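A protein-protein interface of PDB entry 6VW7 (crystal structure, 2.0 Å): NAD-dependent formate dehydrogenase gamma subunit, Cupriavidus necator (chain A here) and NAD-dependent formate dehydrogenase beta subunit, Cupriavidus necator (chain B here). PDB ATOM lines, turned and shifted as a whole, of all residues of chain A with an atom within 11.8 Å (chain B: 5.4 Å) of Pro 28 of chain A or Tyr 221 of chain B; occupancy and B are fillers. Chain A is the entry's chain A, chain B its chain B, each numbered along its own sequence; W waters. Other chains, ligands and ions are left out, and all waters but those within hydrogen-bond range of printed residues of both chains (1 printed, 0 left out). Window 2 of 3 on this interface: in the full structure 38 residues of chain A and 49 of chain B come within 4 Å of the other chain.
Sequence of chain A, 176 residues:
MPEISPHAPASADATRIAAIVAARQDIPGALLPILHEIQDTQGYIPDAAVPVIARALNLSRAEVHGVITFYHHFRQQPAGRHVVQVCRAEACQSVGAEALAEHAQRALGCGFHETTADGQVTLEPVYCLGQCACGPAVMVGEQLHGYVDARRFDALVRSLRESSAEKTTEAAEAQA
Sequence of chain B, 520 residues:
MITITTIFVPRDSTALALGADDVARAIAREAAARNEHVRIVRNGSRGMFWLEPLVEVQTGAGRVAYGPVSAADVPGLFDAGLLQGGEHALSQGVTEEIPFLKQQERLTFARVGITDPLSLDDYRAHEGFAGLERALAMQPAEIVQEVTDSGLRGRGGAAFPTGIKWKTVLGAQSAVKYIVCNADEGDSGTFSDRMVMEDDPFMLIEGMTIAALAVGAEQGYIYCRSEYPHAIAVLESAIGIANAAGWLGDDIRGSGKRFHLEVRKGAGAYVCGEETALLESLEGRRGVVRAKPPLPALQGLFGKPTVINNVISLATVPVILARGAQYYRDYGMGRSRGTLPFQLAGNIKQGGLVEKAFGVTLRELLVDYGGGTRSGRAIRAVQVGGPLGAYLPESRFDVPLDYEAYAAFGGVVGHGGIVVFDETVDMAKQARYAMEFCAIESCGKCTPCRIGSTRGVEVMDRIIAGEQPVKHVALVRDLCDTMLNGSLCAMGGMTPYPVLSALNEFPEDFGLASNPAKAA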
ATOM      1  N   ILE A  20      -4.919  19.478  12.353  1.00  0.00           N
ATOM      2  CA  ILE A  20      -5.809  20.623  12.511  1.00  0.00           C
ATOM      3  C   ILE A  20      -6.914  20.300  13.514  1.00  0.00           C
ATOM      4  O   ILE A  20      -7.229  21.098  14.413  1.00  0.00           O
ATOM      5  CB  ILE A  20      -6.398  21.032  11.148  1.00  0.00           C
ATOM      6  CG1 ILE A  20      -5.357  21.753  10.275  1.00  0.00           C
ATOM      7  CG2 ILE A  20      -7.676  21.855  11.336  1.00  0.00           C
ATOM      8  CD1 ILE A  20      -5.803  21.876   8.814  1.00  0.00           C
ATOM      9  N   VAL A  21      -7.510  19.116  13.370  1.00  0.00           N
ATOM     10  CA  VAL A  21      -8.581  18.687  14.269  1.00  0.00           C
ATOM     11  C   VAL A  21      -8.040  18.507  15.681  1.00  0.00           C
ATOM     12  O   VAL A  21      -8.648  18.959  16.660  1.00  0.00           O
ATOM     13  CB  VAL A  21      -9.209  17.386  13.732  1.00  0.00           C
ATOM     14  CG1 VAL A  21     -10.143  16.766  14.742  1.00  0.00           C
ATOM     15  CG2 VAL A  21      -9.898  17.620  12.384  1.00  0.00           C
ATOM     16  N   ALA A  22      -6.869  17.858  15.803  1.00  0.00           N
ATOM     17  CA  ALA A  22      -6.310  17.544  17.115  1.00  0.00           C
ATOM     18  C   ALA A  22      -5.932  18.801  17.892  1.00  0.00           C
ATOM     19  O   ALA A  22      -6.022  18.814  19.127  1.00  0.00           O
ATOM     20  CB  ALA A  22      -5.086  16.632  16.970  1.00  0.00           C
ATOM     21  N   ALA A  23      -5.466  19.842  17.202  1.00  0.00           N
ATOM     22  CA  ALA A  23      -5.120  21.087  17.880  1.00  0.00           C
ATOM     23  C   ALA A  23      -6.363  21.808  18.402  1.00  0.00           C
ATOM     24  O   ALA A  23      -6.263  22.617  19.336  1.00  0.00           O
ATOM     25  CB  ALA A  23      -4.363  22.016  16.929  1.00  0.00           C
ATOM     26  N   ARG A  24      -7.522  21.555  17.812  1.00  0.00           N
ATOM     27  CA  ARG A  24      -8.730  22.310  18.140  1.00  0.00           C
ATOM     28  C   ARG A  24      -9.742  21.508  18.940  1.00  0.00           C
ATOM     29  O   ARG A  24     -10.800  22.043  19.300  1.00  0.00           O
ATOM     30  CB  ARG A  24      -9.379  22.834  16.856  1.00  0.00           C
ATOM     31  CG  ARG A  24      -8.556  23.925  16.203  1.00  0.00           C
ATOM     32  CD  ARG A  24      -9.017  24.316  14.807  1.00  0.00           C
ATOM     33  NE  ARG A  24      -8.189  25.418  14.316  1.00  0.00           N
ATOM     34  CZ  ARG A  24      -6.933  25.271  13.906  1.00  0.00           C
ATOM     35  NH1 ARG A  24      -6.375  24.073  13.907  1.00  0.00           N
ATOM     36  NH2 ARG A  24      -6.239  26.318  13.493  1.00  0.00           N
ATOM     37  N   GLN A  25      -9.440  20.254  19.257  1.00  0.00           N
ATOM     38  CA  GLN A  25     -10.506  19.346  19.655  1.00  0.00           C
ATOM     39  C   GLN A  25     -11.078  19.670  21.035  1.00  0.00           C
ATOM     40  O   GLN A  25     -12.176  19.200  21.360  1.00  0.00           O
ATOM     41  CB  GLN A  25      -9.997  17.902  19.584  1.00  0.00           C
ATOM     42  CG  GLN A  25      -8.973  17.529  20.603  1.00  0.00           C
ATOM     43  CD  GLN A  25      -8.650  16.050  20.504  1.00  0.00           C
ATOM     44  OE1 GLN A  25      -8.368  15.550  19.416  1.00  0.00           O
ATOM     45  NE2 GLN A  25      -8.768  15.334  21.610  1.00  0.00           N
ATOM     46  N   ASP A  26     -10.385  20.478  21.841  1.00  0.00           N
ATOM     47  CA  ASP A  26     -10.908  20.884  23.139  1.00  0.00           C
ATOM     48  C   ASP A  26     -11.413  22.326  23.156  1.00  0.00           C
ATOM     49  O   ASP A  26     -11.670  22.867  24.233  1.00  0.00           O
ATOM     50  CB  ASP A  26      -9.849  20.688  24.225  1.00  0.00           C
ATOM     51  CG  ASP A  26      -9.734  19.230  24.674  1.00  0.00           C
ATOM     52  OD1 ASP A  26     -10.519  18.388  24.181  1.00  0.00           O
ATOM     53  OD2 ASP A  26      -8.860  18.927  25.515  1.00  0.00           O
ATOM     54  N   ILE A  27     -11.540  22.969  22.003  1.00  0.00           N
ATOM     55  CA  ILE A  27     -12.092  24.323  21.956  1.00  0.00           C
ATOM     56  C   ILE A  27     -13.611  24.238  22.104  1.00  0.00           C
ATOM     57  O   ILE A  27     -14.246  23.380  21.474  1.00  0.00           O
ATOM     58  CB  ILE A  27     -11.681  25.038  20.662  1.00  0.00           C
ATOM     59  CG1 ILE A  27     -10.166  25.305  20.676  1.00  0.00           C
ATOM     60  CG2 ILE A  27     -12.446  26.335  20.484  1.00  0.00           C
ATOM     61  CD1 ILE A  27      -9.695  26.093  19.522  1.00  0.00           C
ATOM     62  N   PRO A  28     -14.221  25.084  22.934  1.00  0.00           N
ATOM     63  CA  PRO A  28     -15.698  25.127  23.026  1.00  0.00           C
ATOM     64  C   PRO A  28     -16.332  25.407  21.671  1.00  0.00           C
ATOM     65  O   PRO A  28     -16.054  26.430  21.034  1.00  0.00           O
ATOM     66  CB  PRO A  28     -15.955  26.277  24.009  1.00  0.00           C
ATOM     67  CG  PRO A  28     -14.669  26.415  24.809  1.00  0.00           C
ATOM     68  CD  PRO A  28     -13.560  26.016  23.873  1.00  0.00           C
ATOM     69  N   GLY A  29     -17.201  24.498  21.234  1.00  0.00           N
ATOM     70  CA  GLY A  29     -17.812  24.643  19.923  1.00  0.00           C
ATOM     71  C   GLY A  29     -16.796  24.634  18.794  1.00  0.00           C
ATOM     72  O   GLY A  29     -16.841  25.468  17.889  1.00  0.00           O
ATOM     73  N   ALA A  30     -15.909  23.636  18.804  1.00  0.00           N
ATOM     74  CA  ALA A  30     -14.767  23.601  17.899  1.00  0.00           C
ATOM     75  C   ALA A  30     -15.127  23.321  16.442  1.00  0.00           C
ATOM     76  O   ALA A  30     -14.275  23.543  15.583  1.00  0.00           O
ATOM     77  CB  ALA A  30     -13.778  22.519  18.379  1.00  0.00           C
ATOM     78  N   LEU A  31     -16.337  22.840  16.134  1.00  0.00           N
ATOM     79  CA  LEU A  31     -16.590  22.310  14.792  1.00  0.00           C
ATOM     80  C   LEU A  31     -16.389  23.370  13.708  1.00  0.00           C
ATOM     81  O   LEU A  31     -15.693  23.116  12.717  1.00  0.00           O
ATOM     82  CB  LEU A  31     -17.984  21.692  14.695  1.00  0.00           C
ATOM     83  CG  LEU A  31     -18.303  21.049  13.343  1.00  0.00           C
ATOM     84  CD1 LEU A  31     -17.143  20.177  12.872  1.00  0.00           C
ATOM     85  CD2 LEU A  31     -19.585  20.214  13.425  1.00  0.00           C
ATOM     86  N   LEU A  32     -17.024  24.551  13.846  1.00  0.00           N
ATOM     87  CA  LEU A  32     -16.857  25.583  12.819  1.00  0.00           C
ATOM     88  C   LEU A  32     -15.418  26.087  12.699  1.00  0.00           C
ATOM     89  O   LEU A  32     -14.969  26.296  11.559  1.00  0.00           O
ATOM     90  CB  LEU A  32     -17.820  26.761  13.051  1.00  0.00           C
ATOM     91  CG  LEU A  32     -19.103  26.679  12.219  1.00  0.00           C
ATOM     92  CD1 LEU A  32     -19.978  25.575  12.759  1.00  0.00           C
ATOM     93  CD2 LEU A  32     -19.901  28.015  12.171  1.00  0.00           C
ATOM     94  N   PRO A  33     -14.683  26.394  13.788  1.00  0.00           N
ATOM     95  CA  PRO A  33     -13.250  26.721  13.613  1.00  0.00           C
ATOM     96  C   PRO A  33     -12.477  25.618  12.916  1.00  0.00           C
ATOM     97  O   PRO A  33     -11.556  25.900  12.134  1.00  0.00           O
ATOM     98  CB  PRO A  33     -12.760  26.947  15.049  1.00  0.00           C
ATOM     99  CG  PRO A  33     -14.025  27.496  15.758  1.00  0.00           C
ATOM    100  CD  PRO A  33     -15.144  26.671  15.168  1.00  0.00           C
ATOM    101  N   ILE A  34     -12.814  24.356  13.188  1.00  0.00           N
ATOM    102  CA  ILE A  34     -12.130  23.252  12.516  1.00  0.00           C
ATOM    103  C   ILE A  34     -12.449  23.267  11.026  1.00  0.00           C
ATOM    104  O   ILE A  34     -11.553  23.173  10.181  1.00  0.00           O
ATOM    105  CB  ILE A  34     -12.517  21.907  13.160  1.00  0.00           C
ATOM    106  CG1 ILE A  34     -11.840  21.751  14.518  1.00  0.00           C
ATOM    107  CG2 ILE A  34     -12.183  20.736  12.232  1.00  0.00           C
ATOM    108  CD1 ILE A  34     -12.275  20.507  15.295  1.00  0.00           C
ATOM    109  N   LEU A  35     -13.733  23.407  10.683  1.00  0.00           N
ATOM    110  CA  LEU A  35     -14.127  23.400   9.277  1.00  0.00           C
ATOM    111  C   LEU A  35     -13.498  24.570   8.529  1.00  0.00           C
ATOM    112  O   LEU A  35     -13.070  24.418   7.380  1.00  0.00           O
ATOM    113  CB  LEU A  35     -15.657  23.437   9.153  1.00  0.00           C
ATOM    114  CG  LEU A  35     -16.407  22.187   9.639  1.00  0.00           C
ATOM    115  CD1 LEU A  35     -17.956  22.383   9.585  1.00  0.00           C
ATOM    116  CD2 LEU A  35     -16.007  20.980   8.832  1.00  0.00           C
ATOM    117  N   HIS A  36     -13.439  25.747   9.163  1.00  0.00           N
ATOM    118  CA  HIS A  36     -12.758  26.896   8.563  1.00  0.00           C
ATOM    119  C   HIS A  36     -11.278  26.610   8.303  1.00  0.00           C
ATOM    120  O   HIS A  36     -10.744  26.942   7.237  1.00  0.00           O
ATOM    121  CB  HIS A  36     -12.898  28.120   9.466  1.00  0.00           C
ATOM    122  CG  HIS A  36     -14.219  28.823   9.330  1.00  0.00           C
ATOM    123  ND1 HIS A  36     -14.692  29.289   8.122  1.00  0.00           N
ATOM    124  CD2 HIS A  36     -15.162  29.136  10.251  1.00  0.00           C
ATOM    125  CE1 HIS A  36     -15.863  29.875   8.308  1.00  0.00           C
ATOM    126  NE2 HIS A  36     -16.176  29.784   9.588  1.00  0.00           N
ATOM    127  N   ALA A  56     -13.042  12.979  16.969  1.00  0.00           N
ATOM    128  CA  ALA A  56     -12.347  13.858  17.903  1.00  0.00           C
ATOM    129  C   ALA A  56     -13.316  14.691  18.743  1.00  0.00           C
ATOM    130  O   ALA A  56     -13.022  14.985  19.907  1.00  0.00           O
ATOM    131  CB  ALA A  56     -11.392  14.771  17.152  1.00  0.00           C
ATOM    132  N   LEU A  57     -14.453  15.089  18.181  1.00  0.00           N
ATOM    133  CA  LEU A  57     -15.430  15.911  18.891  1.00  0.00           C
ATOM    134  C   LEU A  57     -16.546  15.097  19.541  1.00  0.00           C
ATOM    135  O   LEU A  57     -17.500  15.685  20.077  1.00  0.00           O
ATOM    136  CB  LEU A  57     -16.042  16.941  17.933  1.00  0.00           C
ATOM    137  CG  LEU A  57     -15.054  17.839  17.163  1.00  0.00           C
ATOM    138  CD1 LEU A  57     -15.835  18.958  16.454  1.00  0.00           C
ATOM    139  CD2 LEU A  57     -13.964  18.432  18.057  1.00  0.00           C
ATOM    140  N   LEU A  59     -18.885  13.488  18.106  1.00  0.00           N
ATOM    141  CA  LEU A  59     -20.100  13.780  17.357  1.00  0.00           C
ATOM    142  C   LEU A  59     -20.338  12.648  16.367  1.00  0.00           C
ATOM    143  O   LEU A  59     -19.423  11.890  16.039  1.00  0.00           O
ATOM    144  CB  LEU A  59     -19.992  15.115  16.604  1.00  0.00           C
ATOM    145  CG  LEU A  59     -19.802  16.396  17.415  1.00  0.00           C
ATOM    146  CD1 LEU A  59     -19.576  17.563  16.492  1.00  0.00           C
ATOM    147  CD2 LEU A  59     -21.032  16.649  18.286  1.00  0.00           C
ATOM    148  N   TYR B 178     -21.027  34.652  30.095  1.00  0.00           N
ATOM    149  CA  TYR B 178     -20.397  35.001  28.831  1.00  0.00           C
ATOM    150  C   TYR B 178     -20.877  36.349  28.324  1.00  0.00           C
ATOM    151  O   TYR B 178     -22.014  36.761  28.580  1.00  0.00           O
ATOM    152  CB  TYR B 178     -20.685  33.975  27.744  1.00  0.00           C
ATOM    153  CG  TYR B 178     -20.108  32.601  27.996  1.00  0.00           C
ATOM    154  CD1 TYR B 178     -18.736  32.366  27.887  1.00  0.00           C
ATOM    155  CD2 TYR B 178     -20.938  31.533  28.298  1.00  0.00           C
ATOM    156  CE1 TYR B 178     -18.207  31.100  28.097  1.00  0.00           C
ATOM    157  CE2 TYR B 178     -20.433  30.269  28.494  1.00  0.00           C
ATOM    158  CZ  TYR B 178     -19.059  30.057  28.400  1.00  0.00           C
ATOM    159  OH  TYR B 178     -18.552  28.796  28.610  1.00  0.00           O
ATOM    160  N   ILE B 179     -19.996  37.031  27.588  1.00  0.00           N
ATOM    161  CA  ILE B 179     -20.369  38.151  26.733  1.00  0.00           C
ATOM    162  C   ILE B 179     -20.273  37.663  25.298  1.00  0.00           C
ATOM    163  O   ILE B 179     -19.221  37.154  24.877  1.00  0.00           O
ATOM    164  CB  ILE B 179     -19.464  39.384  26.919  1.00  0.00           C
ATOM    165  CG1 ILE B 179     -19.268  39.752  28.400  1.00  0.00           C
ATOM    166  CG2 ILE B 179     -20.004  40.548  26.086  1.00  0.00           C
ATOM    167  CD1 ILE B 179     -20.568  39.986  29.181  1.00  0.00           C
ATOM    168  N   VAL B 180     -21.354  37.809  24.545  1.00  0.00           N
ATOM    169  CA  VAL B 180     -21.362  37.426  23.142  1.00  0.00           C
ATOM    170  C   VAL B 180     -21.690  38.659  22.324  1.00  0.00           C
ATOM    171  O   VAL B 180     -22.748  39.278  22.514  1.00  0.00           O
ATOM    172  CB  VAL B 180     -22.346  36.283  22.856  1.00  0.00           C
ATOM    173  CG1 VAL B 180     -22.521  36.095  21.342  1.00  0.00           C
ATOM    174  CG2 VAL B 180     -21.846  34.991  23.507  1.00  0.00           C
ATOM    175  N   CYS B 181     -20.779  39.028  21.423  1.00  0.00           N
ATOM    176  CA  CYS B 181     -21.021  40.128  20.511  1.00  0.00           C
ATOM    177  C   CYS B 181     -21.565  39.572  19.203  1.00  0.00           C
ATOM    178  O   CYS B 181     -20.919  38.735  18.564  1.00  0.00           O
ATOM    179  CB  CYS B 181     -19.750  40.941  20.269  1.00  0.00           C
ATOM    180  SG  CYS B 181     -19.963  42.129  18.971  1.00  0.00           S
ATOM    181  N   MET B 208     -17.060  45.349  25.466  1.00  0.00           N
ATOM    182  CA  MET B 208     -17.253  43.986  25.957  1.00  0.00           C
ATOM    183  C   MET B 208     -16.585  43.771  27.309  1.00  0.00           C
ATOM    184  O   MET B 208     -17.092  43.005  28.130  1.00  0.00           O
ATOM    185  CB  MET B 208     -16.717  42.984  24.932  1.00  0.00           C
ATOM    186  CG  MET B 208     -17.469  43.031  23.623  1.00  0.00           C
ATOM    187  SD  MET B 208     -16.928  41.821  22.400  1.00  0.00           S
ATOM    188  CE  MET B 208     -17.507  40.271  23.133  1.00  0.00           C
ATOM    189  N   GLN B 219     -15.209  35.503  29.841  1.00  0.00           N
ATOM    190  CA  GLN B 219     -14.940  35.041  28.489  1.00  0.00           C
ATOM    191  C   GLN B 219     -15.916  35.698  27.532  1.00  0.00           C
ATOM    192  O   GLN B 219     -17.122  35.741  27.803  1.00  0.00           O
ATOM    193  CB  GLN B 219     -15.060  33.503  28.380  1.00  0.00           C
ATOM    194  CG  GLN B 219     -14.870  32.997  26.943  1.00  0.00           C
ATOM    195  CD  GLN B 219     -13.431  33.112  26.479  1.00  0.00           C
ATOM    196  OE1 GLN B 219     -12.523  32.697  27.185  1.00  0.00           O
ATOM    197  NE2 GLN B 219     -13.211  33.711  25.302  1.00  0.00           N
ATOM    198  N   GLY B 220     -15.399  36.176  26.407  1.00  0.00           N
ATOM    199  CA  GLY B 220     -16.229  36.785  25.389  1.00  0.00           C
ATOM    200  C   GLY B 220     -15.968  36.181  24.023  1.00  0.00           C
ATOM    201  O   GLY B 220     -14.886  35.657  23.736  1.00  0.00           O
ATOM    202  N   TYR B 221     -16.979  36.270  23.176  1.00  0.00           N
ATOM    203  CA  TYR B 221     -16.891  35.779  21.809  1.00  0.00           C
ATOM    204  C   TYR B 221     -17.459  36.831  20.881  1.00  0.00           C
ATOM    205  O   TYR B 221     -18.563  37.328  21.109  1.00  0.00           O
ATOM    206  CB  TYR B 221     -17.660  34.467  21.627  1.00  0.00           C
ATOM    207  CG  TYR B 221     -17.063  33.320  22.391  1.00  0.00           C
ATOM    208  CD1 TYR B 221     -15.999  32.606  21.870  1.00  0.00           C
ATOM    209  CD2 TYR B 221     -17.567  32.941  23.633  1.00  0.00           C
ATOM    210  CE1 TYR B 221     -15.429  31.557  22.569  1.00  0.00           C
ATOM    211  CE2 TYR B 221     -17.010  31.894  24.334  1.00  0.00           C
ATOM    212  CZ  TYR B 221     -15.933  31.210  23.797  1.00  0.00           C
ATOM    213  OH  TYR B 221     -15.365  30.160  24.480  1.00  0.00           O
ATOM    214  N   ILE B 222     -16.732  37.143  19.821  1.00  0.00           N
ATOM    215  CA  ILE B 222     -17.266  37.975  18.758  1.00  0.00           C
ATOM    216  C   ILE B 222     -17.592  37.072  17.576  1.00  0.00           C
ATOM    217  O   ILE B 222     -16.692  36.466  16.979  1.00  0.00           O
ATOM    218  CB  ILE B 222     -16.284  39.084  18.355  1.00  0.00           C
ATOM    219  CG1 ILE B 222     -15.929  39.948  19.564  1.00  0.00           C
ATOM    220  CG2 ILE B 222     -16.895  39.914  17.254  1.00  0.00           C
ATOM    221  CD1 ILE B 222     -14.712  40.920  19.298  1.00  0.00           C
ATOM    222  N   TYR B 223     -18.872  36.983  17.224  1.00  0.00           N
ATOM    223  CA  TYR B 223     -19.303  36.136  16.115  1.00  0.00           C
ATOM    224  C   TYR B 223     -19.443  37.036  14.894  1.00  0.00           C
ATOM    225  O   TYR B 223     -20.412  37.795  14.781  1.00  0.00           O
ATOM    226  CB  TYR B 223     -20.601  35.408  16.461  1.00  0.00           C
ATOM    227  CG  TYR B 223     -21.059  34.418  15.410  1.00  0.00           C
ATOM    228  CD1 TYR B 223     -21.844  34.821  14.331  1.00  0.00           C
ATOM    229  CD2 TYR B 223     -20.700  33.072  15.495  1.00  0.00           C
ATOM    230  CE1 TYR B 223     -22.254  33.905  13.358  1.00  0.00           C
ATOM    231  CE2 TYR B 223     -21.105  32.152  14.534  1.00  0.00           C
ATOM    232  CZ  TYR B 223     -21.895  32.574  13.468  1.00  0.00           C
ATOM    233  OH  TYR B 223     -22.321  31.656  12.513  1.00  0.00           O
ATOM    234  N   LEU B 261     -11.030  37.187  25.153  1.00  0.00           N
ATOM    235  CA  LEU B 261     -11.909  37.490  24.046  1.00  0.00           C
ATOM    236  C   LEU B 261     -11.412  36.750  22.819  1.00  0.00           C
ATOM    237  O   LEU B 261     -10.204  36.686  22.583  1.00  0.00           O
ATOM    238  CB  LEU B 261     -11.894  38.998  23.808  1.00  0.00           C
ATOM    239  CG  LEU B 261     -12.898  39.705  22.967  1.00  0.00           C
ATOM    240  CD1 LEU B 261     -14.256  39.359  23.579  1.00  0.00           C
ATOM    241  CD2 LEU B 261     -12.563  41.204  23.057  1.00  0.00           C
ATOM    242  N   GLU B 262     -12.321  36.180  22.037  1.00  0.00           N
ATOM    243  CA  GLU B 262     -11.858  35.601  20.787  1.00  0.00           C
ATOM    244  C   GLU B 262     -12.911  35.803  19.715  1.00  0.00           C
ATOM    245  O   GLU B 262     -14.100  35.997  20.001  1.00  0.00           O
ATOM    246  CB  GLU B 262     -11.491  34.122  20.956  1.00  0.00           C
ATOM    247  CG  GLU B 262     -12.620  33.156  20.975  1.00  0.00           C
ATOM    248  CD  GLU B 262     -12.158  31.732  21.323  1.00  0.00           C
ATOM    249  OE1 GLU B 262     -11.583  31.544  22.417  1.00  0.00           O
ATOM    250  OE2 GLU B 262     -12.365  30.803  20.510  1.00  0.00           O
ATOM    251  N   ARG B 264     -14.950  34.483  16.389  1.00  0.00           N
ATOM    252  CA  ARG B 264     -15.443  33.304  15.702  1.00  0.00           C
ATOM    253  C   ARG B 264     -15.998  33.730  14.357  1.00  0.00           C
ATOM    254  O   ARG B 264     -16.756  34.706  14.270  1.00  0.00           O
ATOM    255  CB  ARG B 264     -16.516  32.586  16.529  1.00  0.00           C
ATOM    256  CG  ARG B 264     -15.991  31.975  17.830  1.00  0.00           C
ATOM    257  CD  ARG B 264     -14.957  30.885  17.561  1.00  0.00           C
ATOM    258  NE  ARG B 264     -14.512  30.232  18.789  1.00  0.00           N
ATOM    259  CZ  ARG B 264     -15.117  29.198  19.371  1.00  0.00           C
ATOM    260  NH1 ARG B 264     -16.217  28.678  18.843  1.00  0.00           N
ATOM    261  NH2 ARG B 264     -14.611  28.679  20.490  1.00  0.00           N
ATOM    262  N   LEU B 282     -22.079  29.079  17.431  1.00  0.00           N
ATOM    263  CA  LEU B 282     -20.937  29.140  18.344  1.00  0.00           C
ATOM    264  C   LEU B 282     -20.667  27.789  18.988  1.00  0.00           C
ATOM    265  O   LEU B 282     -19.509  27.433  19.247  1.00  0.00           O
ATOM    266  CB  LEU B 282     -21.195  30.179  19.437  1.00  0.00           C
ATOM    267  CG  LEU B 282     -20.949  31.616  19.021  1.00  0.00           C
ATOM    268  CD1 LEU B 282     -21.410  32.572  20.113  1.00  0.00           C
ATOM    269  CD2 LEU B 282     -19.456  31.779  18.720  1.00  0.00           C
ATOM    270  N   LEU B 301     -25.167  30.728  25.930  1.00  0.00           N
ATOM    271  CA  LEU B 301     -24.056  29.938  25.414  1.00  0.00           C
ATOM    272  C   LEU B 301     -23.715  28.814  26.392  1.00  0.00           C
ATOM    273  O   LEU B 301     -23.420  29.067  27.566  1.00  0.00           O
ATOM    274  CB  LEU B 301     -22.848  30.841  25.163  1.00  0.00           C
ATOM    275  CG  LEU B 301     -21.675  30.183  24.445  1.00  0.00           C
ATOM    276  CD1 LEU B 301     -22.094  29.694  23.065  1.00  0.00           C
ATOM    277  CD2 LEU B 301     -20.506  31.165  24.323  1.00  0.00           C
ATOM    278  N   PHE B 302     -23.766  27.570  25.909  1.00  0.00           N
ATOM    279  CA  PHE B 302     -23.575  26.380  26.749  1.00  0.00           C
ATOM    280  C   PHE B 302     -24.501  26.408  27.959  1.00  0.00           C
ATOM    281  O   PHE B 302     -24.158  25.914  29.035  1.00  0.00           O
ATOM    282  CB  PHE B 302     -22.105  26.233  27.179  1.00  0.00           C
ATOM    283  CG  PHE B 302     -21.165  26.266  26.031  1.00  0.00           C
ATOM    284  CD1 PHE B 302     -21.189  25.253  25.084  1.00  0.00           C
ATOM    285  CD2 PHE B 302     -20.290  27.325  25.854  1.00  0.00           C
ATOM    286  CE1 PHE B 302     -20.347  25.291  23.993  1.00  0.00           C
ATOM    287  CE2 PHE B 302     -19.452  27.373  24.766  1.00  0.00           C
ATOM    288  CZ  PHE B 302     -19.480  26.351  23.833  1.00  0.00           C
HETATM  289  O   HOH W   1     -18.522  26.612  16.189  1.00  0.00           O
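O of Pro 28 of chain A lies within hydrogen-bond range of NH2 of Arg 264 of chain B, at 2.7 Å. NH1 of Arg 264 of chain B sits at hydrogen-bond distance from O of Gly 29 of chain A (3.4 Å).
O of Ile 179 of chain B sits at hydrogen-bond distance from N of Tyr 221 of chain B (2.9 Å). The backbone NH (N) of Cys 181 of chain B sits at hydrogen-bond distance from the backbone carbonyl oxygen (O) of Tyr 221 of chain B. The side-chain carboxylate of Glu 262 of chain B is in salt-bridge range of the guanidinium group of Arg 264 of chain B (2.8 Å). O of Ile 222 of chain B lies within hydrogen-bond range of N of Arg 264 of chain B, 2.7 Å away.
Among the printed residues, merely in contact across the chains: Ile 27 of chain A with Arg 264 of chain B (3.2 Å), Pro 28 of chain A with Tyr 221 of chain B (3.8 Å), Pro 28 of chain A with Phe 302 of chain B (3.5 Å), Gly 29 of chain A with Leu 282 of chain B (3.3 Å), Gly 29 of chain A with Phe 302 of chain B (3.9 Å) and Pro 33 of chain A with Arg 264 of chain B (3.95 Å).
Of the printed residues of chain B, Pro 28 of chain A touches Tyr 221, Arg 264 and Phe 302. Tyr 221 of chain B touches one residue of chain A. No residue of chain A comes within 4 Å of Tyr 178 of chain B. No residue of chain A comes within 4 Å of Gly 220 of chain B. No residue of chain A comes within 4 Å of Ile 222 of chain B. No residue of chain A comes within 4 Å of Glu 262 of chain B. Of the printed residues of chain B, Pro 33 of chain A touches Arg 264 (3.95 Å). Of the printed residues of chain B, Gly 29 of chain A touches Arg 264 (3.4 Å), Leu 282 (3.3 Å) and Phe 302 (3.9 Å). Tyr 223 of chain B touches none of the printed residues of chain A. The nearest residue of chain A that does not touch Tyr 221 of chain B is Ile 27 of chain A (6.3 Å). The nearest printed residue of chain B that does not touch Gly 29 of chain A is Tyr 221 of chain B (6.8 Å).
Of the 20 printed residues of chain A, 4 touch a printed residue of chain B. Hydrophobic or aromatic side chains of chain A that line the printed part of chain B: Ile 27, Pro 28 and Pro 33. Along chain A the printed residues that touch a printed residue of chain B span positions 27 to 33. Among the printed residues, 8 pairs touch across the chains.
Water W1 lies within hydrogen-bond range of the backbone carbonyl oxygen of Gly 29 of chain A, the backbone carbonyl oxygen of Leu 282 of chain B and the backbone NH of Leu 32 of chain A.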
